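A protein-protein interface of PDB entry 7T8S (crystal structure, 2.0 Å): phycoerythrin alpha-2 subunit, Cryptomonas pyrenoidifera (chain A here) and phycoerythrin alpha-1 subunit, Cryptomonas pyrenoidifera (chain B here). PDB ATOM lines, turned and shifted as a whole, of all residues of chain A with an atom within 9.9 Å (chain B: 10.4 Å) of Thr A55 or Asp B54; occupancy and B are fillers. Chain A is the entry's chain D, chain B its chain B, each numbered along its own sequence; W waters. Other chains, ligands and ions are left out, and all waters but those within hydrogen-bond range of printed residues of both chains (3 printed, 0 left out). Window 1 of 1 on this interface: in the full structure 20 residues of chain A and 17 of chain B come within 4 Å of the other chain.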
ATOM      1  N   ILE A  49     -22.198  -5.843 -17.948  1.00  0.00           N
ATOM      2  CA  ILE A  49     -21.554  -6.280 -19.184  1.00  0.00           C
ATOM      3  C   ILE A  49     -20.237  -6.953 -18.813  1.00  0.00           C
ATOM      4  O   ILE A  49     -19.409  -6.363 -18.109  1.00  0.00           O
ATOM      5  CB  ILE A  49     -21.325  -5.095 -20.138  1.00  0.00           C
ATOM      6  CG1 ILE A  49     -22.631  -4.332 -20.398  1.00  0.00           C
ATOM      7  CG2 ILE A  49     -20.736  -5.582 -21.452  1.00  0.00           C
ATOM      8  CD1 ILE A  49     -23.766  -5.204 -20.932  1.00  0.00           C
ATOM      9  N   ALA A  50     -20.033  -8.181 -19.294  1.00  0.00           N
ATOM     10  CA  ALA A  50     -18.860  -8.971 -18.940  1.00  0.00           C
ATOM     11  C   ALA A  50     -18.238  -9.575 -20.189  1.00  0.00           C
ATOM     12  O   ALA A  50     -18.942 -10.122 -21.044  1.00  0.00           O
ATOM     13  CB  ALA A  50     -19.219 -10.081 -17.952  1.00  0.00           C
ATOM     14  N   VAL A  51     -16.911  -9.488 -20.277  1.00  0.00           N
ATOM     15  CA  VAL A  51     -16.142 -10.008 -21.405  1.00  0.00           C
ATOM     16  C   VAL A  51     -15.110 -10.989 -20.869  1.00  0.00           C
ATOM     17  O   VAL A  51     -14.350 -10.659 -19.949  1.00  0.00           O
ATOM     18  CB  VAL A  51     -15.470  -8.874 -22.201  1.00  0.00           C
ATOM     19  CG1 VAL A  51     -14.545  -9.439 -23.291  1.00  0.00           C
ATOM     20  CG2 VAL A  51     -16.533  -7.973 -22.812  1.00  0.00           C
ATOM     21  N   SER A  52     -15.098 -12.194 -21.432  1.00  0.00           N
ATOM     22  CA  SER A  52     -14.238 -13.263 -20.957  1.00  0.00           C
ATOM     23  C   SER A  52     -12.806 -13.099 -21.458  1.00  0.00           C
ATOM     24  O   SER A  52     -12.531 -12.401 -22.441  1.00  0.00           O
ATOM     25  CB  SER A  52     -14.767 -14.622 -21.417  1.00  0.00           C
ATOM     26  OG  SER A  52     -14.626 -14.759 -22.828  1.00  0.00           O
ATOM     27  N   ALA A  53     -11.890 -13.797 -20.778  1.00  0.00           N
ATOM     28  CA  ALA A  53     -10.501 -13.839 -21.226  1.00  0.00           C
ATOM     29  C   ALA A  53     -10.384 -14.507 -22.593  1.00  0.00           C
ATOM     30  O   ALA A  53      -9.559 -14.107 -23.421  1.00  0.00           O
ATOM     31  CB  ALA A  53      -9.642 -14.578 -20.195  1.00  0.00           C
ATOM     32  N   THR A  54     -11.196 -15.536 -22.838  1.00  0.00           N
ATOM     33  CA  THR A  54     -11.194 -16.205 -24.134  1.00  0.00           C
ATOM     34  C   THR A  54     -11.548 -15.230 -25.252  1.00  0.00           C
ATOM     35  O   THR A  54     -10.889 -15.193 -26.299  1.00  0.00           O
ATOM     36  CB  THR A  54     -12.177 -17.375 -24.094  1.00  0.00           C
ATOM     37  OG1 THR A  54     -11.757 -18.314 -23.095  1.00  0.00           O
ATOM     38  CG2 THR A  54     -12.277 -18.070 -25.457  1.00  0.00           C
ATOM     39  N   THR A  55     -12.599 -14.435 -25.048  1.00  0.00           N
ATOM     40  CA  THR A  55     -12.981 -13.451 -26.052  1.00  0.00           C
ATOM     41  C   THR A  55     -11.861 -12.436 -26.266  1.00  0.00           C
ATOM     42  O   THR A  55     -11.472 -12.152 -27.404  1.00  0.00           O
ATOM     43  CB  THR A  55     -14.276 -12.760 -25.621  1.00  0.00           C
ATOM     44  OG1 THR A  55     -15.344 -13.716 -25.597  1.00  0.00           O
ATOM     45  CG2 THR A  55     -14.631 -11.624 -26.568  1.00  0.00           C
ATOM     46  N   ALA A  56     -11.305 -11.906 -25.175  1.00  0.00           N
ATOM     47  CA  ALA A  56     -10.222 -10.934 -25.292  1.00  0.00           C
ATOM     48  C   ALA A  56      -9.026 -11.532 -26.017  1.00  0.00           C
ATOM     49  O   ALA A  56      -8.401 -10.869 -26.853  1.00  0.00           O
ATOM     50  CB  ALA A  56      -9.803 -10.443 -23.906  1.00  0.00           C
ATOM     51  N   ASP A  57      -8.687 -12.781 -25.704  1.00  0.00           N
ATOM     52  CA  ASP A  57      -7.591 -13.437 -26.406  1.00  0.00           C
ATOM     53  C   ASP A  57      -7.937 -13.663 -27.871  1.00  0.00           C
ATOM     54  O   ASP A  57      -7.069 -13.568 -28.745  1.00  0.00           O
ATOM     55  CB  ASP A  57      -7.257 -14.765 -25.729  1.00  0.00           C
ATOM     56  CG  ASP A  57      -6.056 -15.436 -26.351  1.00  0.00           C
ATOM     57  OD1 ASP A  57      -4.924 -14.943 -26.135  1.00  0.00           O
ATOM     58  OD2 ASP A  57      -6.248 -16.441 -27.071  1.00  0.00           O
ATOM     59  N   SER A  58      -9.202 -13.962 -28.158  1.00  0.00           N
ATOM     60  CA  SER A  58      -9.608 -14.197 -29.537  1.00  0.00           C
ATOM     61  C   SER A  58      -9.479 -12.930 -30.371  1.00  0.00           C
ATOM     62  O   SER A  58      -8.974 -12.973 -31.501  1.00  0.00           O
ATOM     63  CB  SER A  58     -11.040 -14.723 -29.558  1.00  0.00           C
ATOM     64  OG  SER A  58     -11.551 -14.780 -30.870  1.00  0.00           O
ATOM     65  N   VAL A  59      -9.910 -11.788 -29.828  1.00  0.00           N
ATOM     66  CA  VAL A  59      -9.812 -10.529 -30.566  1.00  0.00           C
ATOM     67  C   VAL A  59      -8.352 -10.172 -30.811  1.00  0.00           C
ATOM     68  O   VAL A  59      -7.981  -9.725 -31.903  1.00  0.00           O
ATOM     69  CB  VAL A  59     -10.556  -9.411 -29.812  1.00  0.00           C
ATOM     70  CG1 VAL A  59     -10.366  -8.067 -30.497  1.00  0.00           C
ATOM     71  CG2 VAL A  59     -12.039  -9.749 -29.723  1.00  0.00           C
ATOM     72  N   LEU A  60      -7.496 -10.377 -29.806  1.00  0.00           N
ATOM     73  CA  LEU A  60      -6.075 -10.100 -29.991  1.00  0.00           C
ATOM     74  C   LEU A  60      -5.494 -10.968 -31.101  1.00  0.00           C
ATOM     75  O   LEU A  60      -4.819 -10.467 -32.009  1.00  0.00           O
ATOM     76  CB  LEU A  60      -5.328 -10.335 -28.682  1.00  0.00           C
ATOM     77  CG  LEU A  60      -3.809 -10.211 -28.744  1.00  0.00           C
ATOM     78  CD1 LEU A  60      -3.397  -8.780 -29.096  1.00  0.00           C
ATOM     79  CD2 LEU A  60      -3.211 -10.636 -27.411  1.00  0.00           C
ATOM     80  N   GLN A  61      -5.804 -12.267 -31.075  1.00  0.00           N
ATOM     81  CA  GLN A  61      -5.209 -13.202 -32.026  1.00  0.00           C
ATOM     82  C   GLN A  61      -5.666 -12.923 -33.452  1.00  0.00           C
ATOM     83  O   GLN A  61      -4.901 -13.145 -34.402  1.00  0.00           O
ATOM     84  CB  GLN A  61      -5.558 -14.631 -31.608  1.00  0.00           C
ATOM     85  CG  GLN A  61      -4.861 -15.729 -32.413  1.00  0.00           C
ATOM     86  CD  GLN A  61      -5.635 -16.137 -33.652  1.00  0.00           C
ATOM     87  OE1 GLN A  61      -6.836 -15.878 -33.759  1.00  0.00           O
ATOM     88  NE2 GLN A  61      -4.951 -16.793 -34.593  1.00  0.00           N
ATOM     89  N   GLN A  62      -6.890 -12.426 -33.625  1.00  0.00           N
ATOM     90  CA  GLN A  62      -7.406 -12.065 -34.942  1.00  0.00           C
ATOM     91  C   GLN A  62      -7.081 -10.627 -35.319  1.00  0.00           C
ATOM     92  O   GLN A  62      -7.280 -10.247 -36.475  1.00  0.00           O
ATOM     93  CB  GLN A  62      -8.924 -12.286 -35.002  1.00  0.00           C
ATOM     94  CG  GLN A  62      -9.319 -13.766 -34.886  1.00  0.00           C
ATOM     95  CD  GLN A  62     -10.825 -13.996 -34.886  1.00  0.00           C
ATOM     96  OE1 GLN A  62     -11.564 -13.399 -35.663  1.00  0.00           O
ATOM     97  NE2 GLN A  62     -11.281 -14.859 -33.991  1.00  0.00           N
ATOM     98  N   THR A  63      -6.563  -9.837 -34.384  1.00  0.00           N
ATOM     99  CA  THR A  63      -6.109  -8.485 -34.684  1.00  0.00           C
ATOM    100  C   THR A  63      -4.619  -8.449 -35.010  1.00  0.00           C
ATOM    101  O   THR A  63      -4.201  -7.752 -35.941  1.00  0.00           O
ATOM    102  CB  THR A  63      -6.389  -7.560 -33.495  1.00  0.00           C
ATOM    103  OG1 THR A  63      -7.797  -7.518 -33.247  1.00  0.00           O
ATOM    104  CG2 THR A  63      -5.873  -6.142 -33.769  1.00  0.00           C
ATOM    105  N   ALA B  49     -12.497 -23.691 -26.277  1.00  0.00           N
ATOM    106  CA  ALA B  49     -13.456 -23.628 -25.189  1.00  0.00           C
ATOM    107  C   ALA B  49     -14.383 -22.443 -25.387  1.00  0.00           C
ATOM    108  O   ALA B  49     -13.969 -21.384 -25.869  1.00  0.00           O
ATOM    109  CB  ALA B  49     -12.754 -23.509 -23.833  1.00  0.00           C
ATOM    110  N   VAL B  50     -15.642 -22.641 -25.022  1.00  0.00           N
ATOM    111  CA  VAL B  50     -16.646 -21.589 -25.007  1.00  0.00           C
ATOM    112  C   VAL B  50     -17.350 -21.684 -23.663  1.00  0.00           C
ATOM    113  O   VAL B  50     -17.846 -22.757 -23.295  1.00  0.00           O
ATOM    114  CB  VAL B  50     -17.649 -21.728 -26.163  1.00  0.00           C
ATOM    115  CG1 VAL B  50     -18.717 -20.630 -26.077  1.00  0.00           C
ATOM    116  CG2 VAL B  50     -16.919 -21.706 -27.512  1.00  0.00           C
ATOM    117  N   SER B  51     -17.365 -20.585 -22.919  1.00  0.00           N
ATOM    118  CA  SER B  51     -18.012 -20.575 -21.616  1.00  0.00           C
ATOM    119  C   SER B  51     -19.527 -20.519 -21.772  1.00  0.00           C
ATOM    120  O   SER B  51     -20.060 -20.078 -22.793  1.00  0.00           O
ATOM    121  CB  SER B  51     -17.532 -19.384 -20.791  1.00  0.00           C
ATOM    122  OG  SER B  51     -18.030 -18.170 -21.334  1.00  0.00           O
ATOM    123  N   GLU B  52     -20.226 -20.978 -20.734  1.00  0.00           N
ATOM    124  CA  GLU B  52     -21.683 -20.908 -20.754  1.00  0.00           C
ATOM    125  C   GLU B  52     -22.155 -19.464 -20.767  1.00  0.00           C
ATOM    126  O   GLU B  52     -23.146 -19.130 -21.431  1.00  0.00           O
ATOM    127  CB  GLU B  52     -22.256 -21.657 -19.555  1.00  0.00           C
ATOM    128  CG  GLU B  52     -21.944 -23.147 -19.599  1.00  0.00           C
ATOM    129  CD  GLU B  52     -22.836 -23.978 -18.699  1.00  0.00           C
ATOM    130  OE1 GLU B  52     -23.819 -23.432 -18.147  1.00  0.00           O
ATOM    131  OE2 GLU B  52     -22.550 -25.185 -18.557  1.00  0.00           O
ATOM    132  N   ALA B  53     -21.452 -18.588 -20.049  1.00  0.00           N
ATOM    133  CA  ALA B  53     -21.821 -17.179 -20.074  1.00  0.00           C
ATOM    134  C   ALA B  53     -21.684 -16.605 -21.482  1.00  0.00           C
ATOM    135  O   ALA B  53     -22.572 -15.887 -21.953  1.00  0.00           O
ATOM    136  CB  ALA B  53     -20.973 -16.399 -19.074  1.00  0.00           C
ATOM    137  N   ASP B  54     -20.597 -16.936 -22.185  1.00  0.00           N
ATOM    138  CA  ASP B  54     -20.437 -16.443 -23.551  1.00  0.00           C
ATOM    139  C   ASP B  54     -21.481 -17.049 -24.484  1.00  0.00           C
ATOM    140  O   ASP B  54     -21.966 -16.377 -25.400  1.00  0.00           O
ATOM    141  CB  ASP B  54     -19.023 -16.732 -24.055  1.00  0.00           C
ATOM    142  CG  ASP B  54     -17.994 -15.730 -23.530  1.00  0.00           C
ATOM    143  OD1 ASP B  54     -16.777 -16.027 -23.612  1.00  0.00           O
ATOM    144  OD2 ASP B  54     -18.406 -14.680 -22.978  1.00  0.00           O
ATOM    145  N   ALA B  55     -21.835 -18.320 -24.282  1.00  0.00           N
ATOM    146  CA  ALA B  55     -22.909 -18.906 -25.078  1.00  0.00           C
ATOM    147  C   ALA B  55     -24.240 -18.204 -24.824  1.00  0.00           C
ATOM    148  O   ALA B  55     -25.063 -18.081 -25.739  1.00  0.00           O
ATOM    149  CB  ALA B  55     -23.033 -20.397 -24.785  1.00  0.00           C
ATOM    150  N   ALA B  56     -24.474 -17.742 -23.592  1.00  0.00           N
ATOM    151  CA  ALA B  56     -25.702 -17.006 -23.310  1.00  0.00           C
ATOM    152  C   ALA B  56     -25.740 -15.692 -24.082  1.00  0.00           C
ATOM    153  O   ALA B  56     -26.809 -15.253 -24.526  1.00  0.00           O
ATOM    154  CB  ALA B  56     -25.830 -16.744 -21.809  1.00  0.00           C
ATOM    155  N   LYS B  57     -24.584 -15.044 -24.249  1.00  0.00           N
ATOM    156  CA  LYS B  57     -24.558 -13.807 -25.023  1.00  0.00           C
ATOM    157  C   LYS B  57     -24.896 -14.072 -26.482  1.00  0.00           C
ATOM    158  O   LYS B  57     -25.585 -13.271 -27.122  1.00  0.00           O
ATOM    159  CB  LYS B  57     -23.193 -13.127 -24.912  1.00  0.00           C
ATOM    160  CG  LYS B  57     -22.857 -12.643 -23.519  1.00  0.00           C
ATOM    161  CD  LYS B  57     -21.557 -11.845 -23.489  1.00  0.00           C
ATOM    162  CE  LYS B  57     -21.768 -10.384 -23.863  1.00  0.00           C
ATOM    163  NZ  LYS B  57     -20.548  -9.547 -23.590  1.00  0.00           N
ATOM    164  N   LYS B  58     -24.403 -15.187 -27.028  1.00  0.00           N
ATOM    165  CA  LYS B  58     -24.702 -15.520 -28.417  1.00  0.00           C
ATOM    166  C   LYS B  58     -26.175 -15.857 -28.596  1.00  0.00           C
ATOM    167  O   LYS B  58     -26.798 -15.452 -29.588  1.00  0.00           O
ATOM    168  CB  LYS B  58     -23.823 -16.684 -28.880  1.00  0.00           C
ATOM    169  CG  LYS B  58     -22.321 -16.418 -28.791  1.00  0.00           C
ATOM    170  CD  LYS B  58     -21.927 -15.140 -29.523  1.00  0.00           C
ATOM    171  CE  LYS B  58     -22.375 -15.150 -30.962  1.00  0.00           C
ATOM    172  NZ  LYS B  58     -21.885 -13.931 -31.680  1.00  0.00           N
ATOM    173  N   LEU B  59     -26.750 -16.591 -27.645  1.00  0.00           N
ATOM    174  CA  LEU B  59     -28.181 -16.868 -27.688  1.00  0.00           C
ATOM    175  C   LEU B  59     -28.992 -15.575 -27.705  1.00  0.00           C
ATOM    176  O   LEU B  59     -29.955 -15.451 -28.472  1.00  0.00           O
ATOM    177  CB  LEU B  59     -28.570 -17.734 -26.491  1.00  0.00           C
ATOM    178  CG  LEU B  59     -30.066 -18.005 -26.345  1.00  0.00           C
ATOM    179  CD1 LEU B  59     -30.567 -18.844 -27.524  1.00  0.00           C
ATOM    180  CD2 LEU B  59     -30.363 -18.686 -25.011  1.00  0.00           C
ATOM    181  N   GLN B  60     -28.606 -14.597 -26.878  1.00  0.00           N
ATOM    182  CA  GLN B  60     -29.322 -13.323 -26.837  1.00  0.00           C
ATOM    183  C   GLN B  60     -29.289 -12.629 -28.195  1.00  0.00           C
ATOM    184  O   GLN B  60     -30.254 -11.956 -28.582  1.00  0.00           O
ATOM    185  CB  GLN B  60     -28.714 -12.416 -25.767  1.00  0.00           C
ATOM    186  CG  GLN B  60     -29.490 -11.130 -25.521  1.00  0.00           C
ATOM    187  CD  GLN B  60     -29.155 -10.025 -26.518  1.00  0.00           C
ATOM    188  OE1 GLN B  60     -28.097 -10.029 -27.140  1.00  0.00           O
ATOM    189  NE2 GLN B  60     -30.063  -9.073 -26.667  1.00  0.00           N
ATOM    190  N   GLU B  61     -28.176 -12.768 -28.922  1.00  0.00           N
ATOM    191  CA  GLU B  61     -28.081 -12.204 -30.266  1.00  0.00           C
ATOM    192  C   GLU B  61     -28.905 -13.007 -31.265  1.00  0.00           C
ATOM    193  O   GLU B  61     -29.570 -12.429 -32.130  1.00  0.00           O
ATOM    194  CB  GLU B  61     -26.617 -12.172 -30.723  1.00  0.00           C
ATOM    195  CG  GLU B  61     -25.732 -11.169 -29.991  1.00  0.00           C
ATOM    196  CD  GLU B  61     -24.277 -11.208 -30.445  1.00  0.00           C
ATOM    197  OE1 GLU B  61     -23.925 -12.048 -31.315  1.00  0.00           O
ATOM    198  OE2 GLU B  61     -23.486 -10.398 -29.915  1.00  0.00           O
ATOM    199  N   PHE B  62     -28.861 -14.340 -31.173  1.00  0.00           N
ATOM    200  CA  PHE B  62     -29.469 -15.186 -32.196  1.00  0.00           C
ATOM    201  C   PHE B  62     -30.992 -15.225 -32.106  1.00  0.00           C
ATOM    202  O   PHE B  62     -31.661 -15.421 -33.125  1.00  0.00           O
ATOM    203  CB  PHE B  62     -28.944 -16.622 -32.084  1.00  0.00           C
ATOM    204  CG  PHE B  62     -27.463 -16.766 -32.325  1.00  0.00           C
ATOM    205  CD1 PHE B  62     -26.730 -15.745 -32.911  1.00  0.00           C
ATOM    206  CD2 PHE B  62     -26.804 -17.931 -31.952  1.00  0.00           C
ATOM    207  CE1 PHE B  62     -25.363 -15.880 -33.130  1.00  0.00           C
ATOM    208  CE2 PHE B  62     -25.440 -18.075 -32.166  1.00  0.00           C
ATOM    209  CZ  PHE B  62     -24.719 -17.050 -32.766  1.00  0.00           C
HETATM  210  O   HOH W   1     -19.301 -12.944 -20.823  1.00  0.00           O
HETATM  211  O   HOH W   2     -22.004  -9.616 -20.643  1.00  0.00           O
HETATM  212  O   HOH W   3     -16.992 -12.623 -23.693  1.00  0.00           O
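Of the 14 printed residues of chain B, 3 touch a printed residue of chain A.
Among the printed residues, no Asp or Glu carboxylate lies within 4 Å of a Lys or Arg side-chain nitrogen of the other chain.
Thr A54 touches Ala B49 (CG2 to O, 3.7 Å).
OG of Ser B51 is in hydrogen-bond range of N of Asp B54 (3.0 Å).
N of Thr A55 sits at hydrogen-bond distance from OG of Ser A52, at 3.0 Å.
Thr A55 touches one residue of chain B.
No residue of chain B comes within 4 Å of Val A51.
Of chain B, only Asp B54 comes within 4 Å of Ser A52.
No residue of chain B comes within 4 Å of Ala A53.
Thr A54 touches just one residue of chain B: Ala B49.
Ala A56 touches none of the printed residues of chain B.
No residue of chain B comes within 4 Å of Ser A58.
No residue of chain A comes within 4 Å of Ser B51.
No residue of chain A comes within 4 Å of Ala B53.
No residue of chain A comes within 4 Å of Ala B55.
Lys B57 touches just one residue of chain A: Ala A50.
Of the printed residues of chain A, Ala B49 touches Thr A54.
Of the printed residues of chain B, Ala A50 touches Lys B57.
The nearest printed residue of chain B that does not touch Ala A50 is Asp B54 (5.0 Å).
Water W3 lies within hydrogen-bond range of OD2 of Asp B54 (2.6 Å), OG1 of Thr A55 (2.7 Å) and N of Ser A52 (3.0 Å).
Water W2 bridges N of Ala A50 (2.8 Å) and NZ of Lys B57 (3.3 Å).
Water W1 bridges the backbone carbonyl oxygen of Ala A50 and the side-chain carboxylate of Asp B54.
OG of Ser A52 lies within hydrogen-bond range of OD1 of Asp B54, 2.6 Å away.
OD1 of Asp B54 is in hydrogen-bond range of OG1 of Thr A55 (3.4 Å).
The backbone carbonyl oxygen (O) of Ala A50 lies within hydrogen-bond range of the side-chain amino group (NZ) of Lys B57.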
